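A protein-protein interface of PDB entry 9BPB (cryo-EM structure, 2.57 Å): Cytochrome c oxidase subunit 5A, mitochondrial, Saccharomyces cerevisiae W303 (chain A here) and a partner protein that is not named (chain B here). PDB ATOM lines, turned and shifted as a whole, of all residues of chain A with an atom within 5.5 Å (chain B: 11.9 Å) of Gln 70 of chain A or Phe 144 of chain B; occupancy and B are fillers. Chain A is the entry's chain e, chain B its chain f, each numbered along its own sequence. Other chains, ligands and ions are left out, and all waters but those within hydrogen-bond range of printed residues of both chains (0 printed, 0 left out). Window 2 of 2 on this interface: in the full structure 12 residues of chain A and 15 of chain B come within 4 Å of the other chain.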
ATOM      1  N   GLN A  35     -10.047   5.380  16.301  1.00  0.00           N
ATOM      2  CA  GLN A  35      -9.444   4.185  15.727  1.00  0.00           C
ATOM      3  C   GLN A  35     -10.496   3.188  15.275  1.00  0.00           C
ATOM      4  O   GLN A  35     -10.423   2.676  14.153  1.00  0.00           O
ATOM      5  CB  GLN A  35      -8.491   3.532  16.740  1.00  0.00           C
ATOM      6  CG  GLN A  35      -7.563   4.514  17.433  1.00  0.00           C
ATOM      7  CD  GLN A  35      -6.763   3.875  18.548  1.00  0.00           C
ATOM      8  OE1 GLN A  35      -6.853   2.669  18.780  1.00  0.00           O
ATOM      9  NE2 GLN A  35      -5.975   4.682  19.249  1.00  0.00           N
ATOM     10  N   GLU A  66      -3.661  14.735  24.327  1.00  0.00           N
ATOM     11  CA  GLU A  66      -3.260  13.307  24.260  1.00  0.00           C
ATOM     12  C   GLU A  66      -4.136  12.541  23.257  1.00  0.00           C
ATOM     13  O   GLU A  66      -3.576  11.709  22.521  1.00  0.00           O
ATOM     14  CB  GLU A  66      -3.271  12.728  25.678  1.00  0.00           C
ATOM     15  CG  GLU A  66      -3.189  11.216  25.737  1.00  0.00           C
ATOM     16  CD  GLU A  66      -1.964  10.611  25.077  1.00  0.00           C
ATOM     17  OE1 GLU A  66      -0.839  10.971  25.473  1.00  0.00           O
ATOM     18  OE2 GLU A  66      -2.142   9.771  24.175  1.00  0.00           O
ATOM     19  N   PRO A  67      -5.468  12.753  23.174  1.00  0.00           N
ATOM     20  CA  PRO A  67      -6.291  12.079  22.153  1.00  0.00           C
ATOM     21  C   PRO A  67      -5.781  12.279  20.716  1.00  0.00           C
ATOM     22  O   PRO A  67      -5.934  11.365  19.919  1.00  0.00           O
ATOM     23  CB  PRO A  67      -7.675  12.747  22.316  1.00  0.00           C
ATOM     24  CG  PRO A  67      -7.454  13.934  23.214  1.00  0.00           C
ATOM     25  CD  PRO A  67      -6.288  13.540  24.092  1.00  0.00           C
ATOM     26  N   GLU A  68      -5.195  13.441  20.424  1.00  0.00           N
ATOM     27  CA  GLU A  68      -4.724  13.810  19.091  1.00  0.00           C
ATOM     28  C   GLU A  68      -3.443  13.073  18.727  1.00  0.00           C
ATOM     29  O   GLU A  68      -3.281  12.623  17.588  1.00  0.00           O
ATOM     30  CB  GLU A  68      -4.514  15.321  19.007  1.00  0.00           C
ATOM     31  CG  GLU A  68      -5.796  16.122  18.948  1.00  0.00           C
ATOM     32  CD  GLU A  68      -5.544  17.613  18.985  1.00  0.00           C
ATOM     33  OE1 GLU A  68      -4.393  18.013  19.255  1.00  0.00           O
ATOM     34  OE2 GLU A  68      -6.493  18.388  18.742  1.00  0.00           O
ATOM     35  N   LYS A  69      -2.513  12.945  19.678  1.00  0.00           N
ATOM     36  CA  LYS A  69      -1.264  12.246  19.390  1.00  0.00           C
ATOM     37  C   LYS A  69      -1.500  10.776  19.074  1.00  0.00           C
ATOM     38  O   LYS A  69      -0.725  10.174  18.323  1.00  0.00           O
ATOM     39  CB  LYS A  69      -0.289  12.403  20.554  1.00  0.00           C
ATOM     40  CG  LYS A  69       0.399  13.758  20.589  1.00  0.00           C
ATOM     41  CD  LYS A  69       1.478  13.823  21.654  1.00  0.00           C
ATOM     42  CE  LYS A  69       0.879  14.013  23.032  1.00  0.00           C
ATOM     43  NZ  LYS A  69       1.917  14.331  24.048  1.00  0.00           N
ATOM     44  N   GLN A  70      -2.555  10.178  19.632  1.00  0.00           N
ATOM     45  CA  GLN A  70      -2.918   8.819  19.245  1.00  0.00           C
ATOM     46  C   GLN A  70      -3.699   8.793  17.941  1.00  0.00           C
ATOM     47  O   GLN A  70      -3.826   7.732  17.320  1.00  0.00           O
ATOM     48  CB  GLN A  70      -3.736   8.151  20.353  1.00  0.00           C
ATOM     49  CG  GLN A  70      -2.963   7.900  21.635  1.00  0.00           C
ATOM     50  CD  GLN A  70      -3.810   7.254  22.709  1.00  0.00           C
ATOM     51  OE1 GLN A  70      -5.008   7.044  22.529  1.00  0.00           O
ATOM     52  NE2 GLN A  70      -3.189   6.935  23.838  1.00  0.00           N
ATOM     53  N   ALA A  71      -4.232   9.942  17.514  1.00  0.00           N
ATOM     54  CA  ALA A  71      -5.011   9.987  16.282  1.00  0.00           C
ATOM     55  C   ALA A  71      -4.114  10.173  15.064  1.00  0.00           C
ATOM     56  O   ALA A  71      -4.288   9.487  14.051  1.00  0.00           O
ATOM     57  CB  ALA A  71      -6.052  11.104  16.361  1.00  0.00           C
ATOM     58  N   VAL A  72      -3.156  11.100  15.142  1.00  0.00           N
ATOM     59  CA  VAL A  72      -2.277  11.349  14.006  1.00  0.00           C
ATOM     60  C   VAL A  72      -1.409  10.130  13.724  1.00  0.00           C
ATOM     61  O   VAL A  72      -1.096   9.832  12.567  1.00  0.00           O
ATOM     62  CB  VAL A  72      -1.429  12.613  14.244  1.00  0.00           C
ATOM     63  CG1 VAL A  72      -2.321  13.837  14.355  1.00  0.00           C
ATOM     64  CG2 VAL A  72      -0.570  12.469  15.490  1.00  0.00           C
ATOM     65  N   TRP A  73      -1.001   9.409  14.771  1.00  0.00           N
ATOM     66  CA  TRP A  73      -0.219   8.196  14.562  1.00  0.00           C
ATOM     67  C   TRP A  73      -1.034   7.128  13.845  1.00  0.00           C
ATOM     68  O   TRP A  73      -0.518   6.442  12.957  1.00  0.00           O
ATOM     69  CB  TRP A  73       0.305   7.660  15.893  1.00  0.00           C
ATOM     70  CG  TRP A  73       1.259   6.516  15.722  1.00  0.00           C
ATOM     71  CD1 TRP A  73       2.620   6.582  15.682  1.00  0.00           C
ATOM     72  CD2 TRP A  73       0.921   5.133  15.557  1.00  0.00           C
ATOM     73  NE1 TRP A  73       3.152   5.329  15.506  1.00  0.00           N
ATOM     74  CE2 TRP A  73       2.129   4.421  15.425  1.00  0.00           C
ATOM     75  CE3 TRP A  73      -0.285   4.425  15.511  1.00  0.00           C
ATOM     76  CZ2 TRP A  73       2.166   3.040  15.250  1.00  0.00           C
ATOM     77  CZ3 TRP A  73      -0.246   3.056  15.334  1.00  0.00           C
ATOM     78  CH2 TRP A  73       0.970   2.378  15.206  1.00  0.00           C
ATOM     79  N   TYR A  74      -2.304   6.966  14.222  1.00  0.00           N
ATOM     80  CA  TYR A  74      -3.119   5.915  13.621  1.00  0.00           C
ATOM     81  C   TYR A  74      -3.366   6.175  12.139  1.00  0.00           C
ATOM     82  O   TYR A  74      -3.311   5.247  11.326  1.00  0.00           O
ATOM     83  CB  TYR A  74      -4.447   5.777  14.361  1.00  0.00           C
ATOM     84  CG  TYR A  74      -5.325   4.703  13.768  1.00  0.00           C
ATOM     85  CD1 TYR A  74      -4.915   3.377  13.756  1.00  0.00           C
ATOM     86  CD2 TYR A  74      -6.554   5.013  13.201  1.00  0.00           C
ATOM     87  CE1 TYR A  74      -5.705   2.390  13.208  1.00  0.00           C
ATOM     88  CE2 TYR A  74      -7.353   4.032  12.651  1.00  0.00           C
ATOM     89  CZ  TYR A  74      -6.922   2.723  12.657  1.00  0.00           C
ATOM     90  OH  TYR A  74      -7.712   1.738  12.110  1.00  0.00           O
ATOM     91  N   LEU B 101       4.612  15.244  13.321  1.00  0.00           N
ATOM     92  CA  LEU B 101       4.800  14.533  14.585  1.00  0.00           C
ATOM     93  C   LEU B 101       4.915  13.020  14.421  1.00  0.00           C
ATOM     94  O   LEU B 101       5.817  12.427  15.037  1.00  0.00           O
ATOM     95  CB  LEU B 101       3.670  14.906  15.550  1.00  0.00           C
ATOM     96  CG  LEU B 101       3.725  14.318  16.961  1.00  0.00           C
ATOM     97  CD1 LEU B 101       5.027  14.678  17.656  1.00  0.00           C
ATOM     98  CD2 LEU B 101       2.537  14.798  17.773  1.00  0.00           C
ATOM     99  N   PRO B 102       4.061  12.333  13.648  1.00  0.00           N
ATOM    100  CA  PRO B 102       4.128  10.861  13.634  1.00  0.00           C
ATOM    101  C   PRO B 102       5.423  10.280  13.085  1.00  0.00           C
ATOM    102  O   PRO B 102       5.749   9.135  13.418  1.00  0.00           O
ATOM    103  CB  PRO B 102       2.927  10.466  12.762  1.00  0.00           C
ATOM    104  CG  PRO B 102       2.593  11.679  11.987  1.00  0.00           C
ATOM    105  CD  PRO B 102       2.896  12.817  12.889  1.00  0.00           C
ATOM    106  N   THR B 103       6.169  11.004  12.247  1.00  0.00           N
ATOM    107  CA  THR B 103       7.436  10.449  11.779  1.00  0.00           C
ATOM    108  C   THR B 103       8.514  10.539  12.852  1.00  0.00           C
ATOM    109  O   THR B 103       9.408   9.690  12.902  1.00  0.00           O
ATOM    110  CB  THR B 103       7.893  11.135  10.487  1.00  0.00           C
ATOM    111  OG1 THR B 103       9.003  10.417   9.931  1.00  0.00           O
ATOM    112  CG2 THR B 103       8.319  12.566  10.741  1.00  0.00           C
ATOM    113  N   ILE B 105       7.863  10.124  16.037  1.00  0.00           N
ATOM    114  CA  ILE B 105       7.553   9.003  16.917  1.00  0.00           C
ATOM    115  C   ILE B 105       8.113   7.707  16.346  1.00  0.00           C
ATOM    116  O   ILE B 105       8.636   6.863  17.082  1.00  0.00           O
ATOM    117  CB  ILE B 105       6.034   8.911  17.148  1.00  0.00           C
ATOM    118  CG1 ILE B 105       5.462  10.286  17.491  1.00  0.00           C
ATOM    119  CG2 ILE B 105       5.721   7.918  18.250  1.00  0.00           C
ATOM    120  CD1 ILE B 105       3.956  10.308  17.596  1.00  0.00           C
ATOM    121  N   ARG B 106       8.022   7.531  15.027  1.00  0.00           N
ATOM    122  CA  ARG B 106       8.516   6.322  14.380  1.00  0.00           C
ATOM    123  C   ARG B 106      10.037   6.247  14.345  1.00  0.00           C
ATOM    124  O   ARG B 106      10.580   5.191  14.003  1.00  0.00           O
ATOM    125  CB  ARG B 106       7.955   6.232  12.957  1.00  0.00           C
ATOM    126  CG  ARG B 106       8.066   4.859  12.309  1.00  0.00           C
ATOM    127  CD  ARG B 106       6.930   3.947  12.729  1.00  0.00           C
ATOM    128  NE  ARG B 106       6.632   2.938  11.721  1.00  0.00           N
ATOM    129  CZ  ARG B 106       5.693   2.012  11.846  1.00  0.00           C
ATOM    130  NH1 ARG B 106       4.944   1.931  12.934  1.00  0.00           N
ATOM    131  NH2 ARG B 106       5.498   1.146  10.859  1.00  0.00           N
ATOM    132  N   GLU B 109      10.773   4.049  17.244  1.00  0.00           N
ATOM    133  CA  GLU B 109      10.199   2.756  16.889  1.00  0.00           C
ATOM    134  C   GLU B 109      11.072   2.039  15.872  1.00  0.00           C
ATOM    135  O   GLU B 109      11.254   0.817  15.946  1.00  0.00           O
ATOM    136  CB  GLU B 109       8.786   2.932  16.337  1.00  0.00           C
ATOM    137  CG  GLU B 109       7.867   3.769  17.198  1.00  0.00           C
ATOM    138  CD  GLU B 109       6.458   3.826  16.644  1.00  0.00           C
ATOM    139  OE1 GLU B 109       6.158   3.056  15.710  1.00  0.00           O
ATOM    140  OE2 GLU B 109       5.656   4.651  17.130  1.00  0.00           O
ATOM    141  N   LYS B 112      14.153   1.031  17.962  1.00  0.00           N
ATOM    142  CA  LYS B 112      13.914  -0.049  18.915  1.00  0.00           C
ATOM    143  C   LYS B 112      14.062  -1.414  18.258  1.00  0.00           C
ATOM    144  O   LYS B 112      14.652  -2.331  18.841  1.00  0.00           O
ATOM    145  CB  LYS B 112      12.525   0.107  19.532  1.00  0.00           C
ATOM    146  CG  LYS B 112      12.143  -0.964  20.538  1.00  0.00           C
ATOM    147  CD  LYS B 112      10.998  -0.495  21.427  1.00  0.00           C
ATOM    148  CE  LYS B 112      10.047   0.424  20.669  1.00  0.00           C
ATOM    149  NZ  LYS B 112       8.765   0.652  21.385  1.00  0.00           N
ATOM    150  N   TYR B 121      19.302   0.427  23.498  1.00  0.00           N
ATOM    151  CA  TYR B 121      18.159   1.319  23.349  1.00  0.00           C
ATOM    152  C   TYR B 121      18.097   2.306  24.505  1.00  0.00           C
ATOM    153  O   TYR B 121      17.721   3.469  24.322  1.00  0.00           O
ATOM    154  CB  TYR B 121      16.861   0.516  23.257  1.00  0.00           C
ATOM    155  CG  TYR B 121      15.629   1.371  23.039  1.00  0.00           C
ATOM    156  CD1 TYR B 121      15.673   2.492  22.220  1.00  0.00           C
ATOM    157  CD2 TYR B 121      14.422   1.057  23.652  1.00  0.00           C
ATOM    158  CE1 TYR B 121      14.555   3.273  22.021  1.00  0.00           C
ATOM    159  CE2 TYR B 121      13.298   1.832  23.457  1.00  0.00           C
ATOM    160  CZ  TYR B 121      13.370   2.939  22.639  1.00  0.00           C
ATOM    161  OH  TYR B 121      12.251   3.716  22.443  1.00  0.00           O
ATOM    162  N   ARG B 132      14.871  15.164  22.899  1.00  0.00           N
ATOM    163  CA  ARG B 132      13.517  14.633  22.777  1.00  0.00           C
ATOM    164  C   ARG B 132      12.543  15.389  23.673  1.00  0.00           C
ATOM    165  O   ARG B 132      11.446  15.758  23.240  1.00  0.00           O
ATOM    166  CB  ARG B 132      13.509  13.142  23.109  1.00  0.00           C
ATOM    167  CG  ARG B 132      12.182  12.470  22.852  1.00  0.00           C
ATOM    168  CD  ARG B 132      12.206  11.028  23.320  1.00  0.00           C
ATOM    169  NE  ARG B 132      12.286  10.915  24.772  1.00  0.00           N
ATOM    170  CZ  ARG B 132      11.345  11.311  25.618  1.00  0.00           C
ATOM    171  NH1 ARG B 132      10.212  11.851  25.197  1.00  0.00           N
ATOM    172  NH2 ARG B 132      11.541  11.153  26.925  1.00  0.00           N
ATOM    173  N   GLY B 136       9.519  17.475  22.306  1.00  0.00           N
ATOM    174  CA  GLY B 136       8.213  17.017  22.721  1.00  0.00           C
ATOM    175  C   GLY B 136       7.795  15.667  22.181  1.00  0.00           C
ATOM    176  O   GLY B 136       6.635  15.284  22.360  1.00  0.00           O
ATOM    177  N   VAL B 137       8.697  14.939  21.531  1.00  0.00           N
ATOM    178  CA  VAL B 137       8.379  13.640  20.945  1.00  0.00           C
ATOM    179  C   VAL B 137       8.047  12.647  22.053  1.00  0.00           C
ATOM    180  O   VAL B 137       8.857  12.450  22.969  1.00  0.00           O
ATOM    181  CB  VAL B 137       9.541  13.121  20.084  1.00  0.00           C
ATOM    182  CG1 VAL B 137       9.217  11.746  19.526  1.00  0.00           C
ATOM    183  CG2 VAL B 137       9.856  14.101  18.967  1.00  0.00           C
ATOM    184  N   PRO B 138       6.878  12.015  22.020  1.00  0.00           N
ATOM    185  CA  PRO B 138       6.587  10.933  22.962  1.00  0.00           C
ATOM    186  C   PRO B 138       6.931   9.566  22.395  1.00  0.00           C
ATOM    187  O   PRO B 138       6.799   9.301  21.199  1.00  0.00           O
ATOM    188  CB  PRO B 138       5.074  11.066  23.180  1.00  0.00           C
ATOM    189  CG  PRO B 138       4.564  11.643  21.902  1.00  0.00           C
ATOM    190  CD  PRO B 138       5.686  12.422  21.257  1.00  0.00           C
ATOM    191  N   LEU B 139       7.387   8.689  23.283  1.00  0.00           N
ATOM    192  CA  LEU B 139       7.632   7.310  22.899  1.00  0.00           C
ATOM    193  C   LEU B 139       6.307   6.589  22.668  1.00  0.00           C
ATOM    194  O   LEU B 139       5.242   7.045  23.092  1.00  0.00           O
ATOM    195  CB  LEU B 139       8.451   6.589  23.970  1.00  0.00           C
ATOM    196  CG  LEU B 139       9.747   7.244  24.455  1.00  0.00           C
ATOM    197  CD1 LEU B 139      10.595   6.237  25.213  1.00  0.00           C
ATOM    198  CD2 LEU B 139      10.536   7.831  23.299  1.00  0.00           C
ATOM    199  N   LYS B 140       6.378   5.452  21.971  1.00  0.00           N
ATOM    200  CA  LYS B 140       5.157   4.706  21.684  1.00  0.00           C
ATOM    201  C   LYS B 140       4.544   4.135  22.955  1.00  0.00           C
ATOM    202  O   LYS B 140       3.325   4.212  23.151  1.00  0.00           O
ATOM    203  CB  LYS B 140       5.429   3.591  20.677  1.00  0.00           C
ATOM    204  CG  LYS B 140       4.187   3.192  19.895  1.00  0.00           C
ATOM    205  CD  LYS B 140       4.281   1.787  19.336  1.00  0.00           C
ATOM    206  CE  LYS B 140       3.002   1.415  18.604  1.00  0.00           C
ATOM    207  NZ  LYS B 140       2.965  -0.024  18.226  1.00  0.00           N
ATOM    208  N   GLU B 141       5.369   3.557  23.831  1.00  0.00           N
ATOM    209  CA  GLU B 141       4.845   2.974  25.063  1.00  0.00           C
ATOM    210  C   GLU B 141       4.180   4.029  25.937  1.00  0.00           C
ATOM    211  O   GLU B 141       3.107   3.792  26.500  1.00  0.00           O
ATOM    212  CB  GLU B 141       5.962   2.272  25.835  1.00  0.00           C
ATOM    213  CG  GLU B 141       6.673   1.179  25.060  1.00  0.00           C
ATOM    214  CD  GLU B 141       7.873   1.694  24.293  1.00  0.00           C
ATOM    215  OE1 GLU B 141       8.162   2.906  24.379  1.00  0.00           O
ATOM    216  OE2 GLU B 141       8.532   0.884  23.608  1.00  0.00           O
ATOM    217  N   GLU B 142       4.807   5.200  26.066  1.00  0.00           N
ATOM    218  CA  GLU B 142       4.206   6.280  26.842  1.00  0.00           C
ATOM    219  C   GLU B 142       2.910   6.762  26.203  1.00  0.00           C
ATOM    220  O   GLU B 142       1.941   7.076  26.903  1.00  0.00           O
ATOM    221  CB  GLU B 142       5.195   7.436  26.982  1.00  0.00           C
ATOM    222  CG  GLU B 142       6.278   7.203  28.021  1.00  0.00           C
ATOM    223  CD  GLU B 142       7.605   7.816  27.623  1.00  0.00           C
ATOM    224  OE1 GLU B 142       7.628   8.601  26.653  1.00  0.00           O
ATOM    225  OE2 GLU B 142       8.622   7.516  28.282  1.00  0.00           O
ATOM    226  N   LEU B 143       2.876   6.829  24.871  1.00  0.00           N
ATOM    227  CA  LEU B 143       1.703   7.352  24.178  1.00  0.00           C
ATOM    228  C   LEU B 143       0.511   6.410  24.305  1.00  0.00           C
ATOM    229  O   LEU B 143      -0.636   6.865  24.393  1.00  0.00           O
ATOM    230  CB  LEU B 143       2.041   7.600  22.708  1.00  0.00           C
ATOM    231  CG  LEU B 143       0.893   7.996  21.784  1.00  0.00           C
ATOM    232  CD1 LEU B 143       0.266   9.288  22.269  1.00  0.00           C
ATOM    233  CD2 LEU B 143       1.377   8.130  20.350  1.00  0.00           C
ATOM    234  N   PHE B 144       0.764   5.104  24.325  1.00  0.00           N
ATOM    235  CA  PHE B 144      -0.280   4.085  24.306  1.00  0.00           C
ATOM    236  C   PHE B 144      -1.252   4.270  23.135  1.00  0.00           C
ATOM    237  O   PHE B 144      -2.447   4.492  23.345  1.00  0.00           O
ATOM    238  CB  PHE B 144      -1.041   4.056  25.625  1.00  0.00           C
ATOM    239  CG  PHE B 144      -0.233   3.568  26.792  1.00  0.00           C
ATOM    240  CD1 PHE B 144      -0.004   2.215  26.975  1.00  0.00           C
ATOM    241  CD2 PHE B 144       0.276   4.462  27.720  1.00  0.00           C
ATOM    242  CE1 PHE B 144       0.731   1.762  28.052  1.00  0.00           C
ATOM    243  CE2 PHE B 144       1.012   4.016  28.800  1.00  0.00           C
ATOM    244  CZ  PHE B 144       1.240   2.662  28.965  1.00  0.00           C
ATOM    245  N   PRO B 145      -0.769   4.187  21.884  1.00  0.00           N
ATOM    246  CA  PRO B 145      -1.725   4.263  20.779  1.00  0.00           C
ATOM    247  C   PRO B 145      -2.168   2.882  20.302  1.00  0.00           C
ATOM    248  O   PRO B 145      -1.543   1.890  20.680  1.00  0.00           O
ATOM    249  CB  PRO B 145      -0.931   4.986  19.698  1.00  0.00           C
ATOM    250  CG  PRO B 145       0.470   4.505  19.911  1.00  0.00           C
ATOM    251  CD  PRO B 145       0.619   4.173  21.389  1.00  0.00           C
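The side-chain amide nitrogen (NE2) of Gln 70 of chain A lies within hydrogen-bond range of the backbone carbonyl oxygen (O) of Leu 143 of chain B, at 2.6 Å.
The backbone carbonyl oxygen (O) of Phe 144 of chain B lies within hydrogen-bond range of the side-chain amide nitrogen (NE2) of Gln 70 of chain A (2.6 Å).
OE2 of Glu 109 of chain B sits at hydrogen-bond distance from NE1 of Trp 73 of chain A (3.1 Å).
The side-chain carboxylate (OE2) of Glu 66 of chain A sits close to the backbone carbonyl oxygen (O) of Leu 143 of chain B (3.3 Å).
The side-chain amide nitrogen (NE2) of Gln 70 of chain A is in hydrogen-bond range of the side-chain carboxylate (OE2) of Glu 66 of chain A (3.0 Å).
OE1 of Glu 109 of chain B is in salt-bridge range of NH1 of Arg 106 of chain B (3.2 Å).
CG of Lys 69 of chain A touches CD2 of Leu 101 of chain B (3.7 Å).
CG of Pro 138 of chain B touches CD of Lys 69 of chain A, at 3.8 Å.
Leu 143 of chain B touches Lys 69 of chain A (CD2 to O, 3.6 Å).
Pro 145 of chain B touches Gln 70 of chain A.
Arg 106 of chain B touches Trp 73 of chain A (NH1 to CZ2, 3.8 Å).
Lys 140 of chain B touches Trp 73 of chain A.
Gln 70 of chain A touches just these residues of chain B: Leu 143 (2.6 Å), Phe 144 (2.6 Å) and Pro 145 (3.9 Å).
Phe 144 of chain B touches just one residue of chain A: Gln 70.
Of the printed residues of chain B, Glu 66 of chain A touches Leu 143.
No residue of chain B comes within 4 Å of Pro 67 of chain A.
No residue of chain B comes within 4 Å of Ala 71 of chain A.
Of the printed residues of chain A, Pro 145 of chain B touches Gln 70 (3.9 Å).
Of the printed residues of chain A, Arg 106 of chain B touches Trp 73 (3.8 Å).
Of the printed residues of chain A, Glu 109 of chain B touches Trp 73.
Printed residues of chain A within 4 Å of Pro 138 of chain B: Lys 69.
Glu 68 of chain A touches none of the printed residues of chain B.
The nearest residue of chain B that does not touch Gln 70 of chain A is Glu 142 of chain B (6.0 Å).
Printed residues of chain B that touch a printed residue of chain A: Leu 101, Arg 106, Glu 109, Pro 138, Lys 140, Leu 143, Phe 144 and Pro 145.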
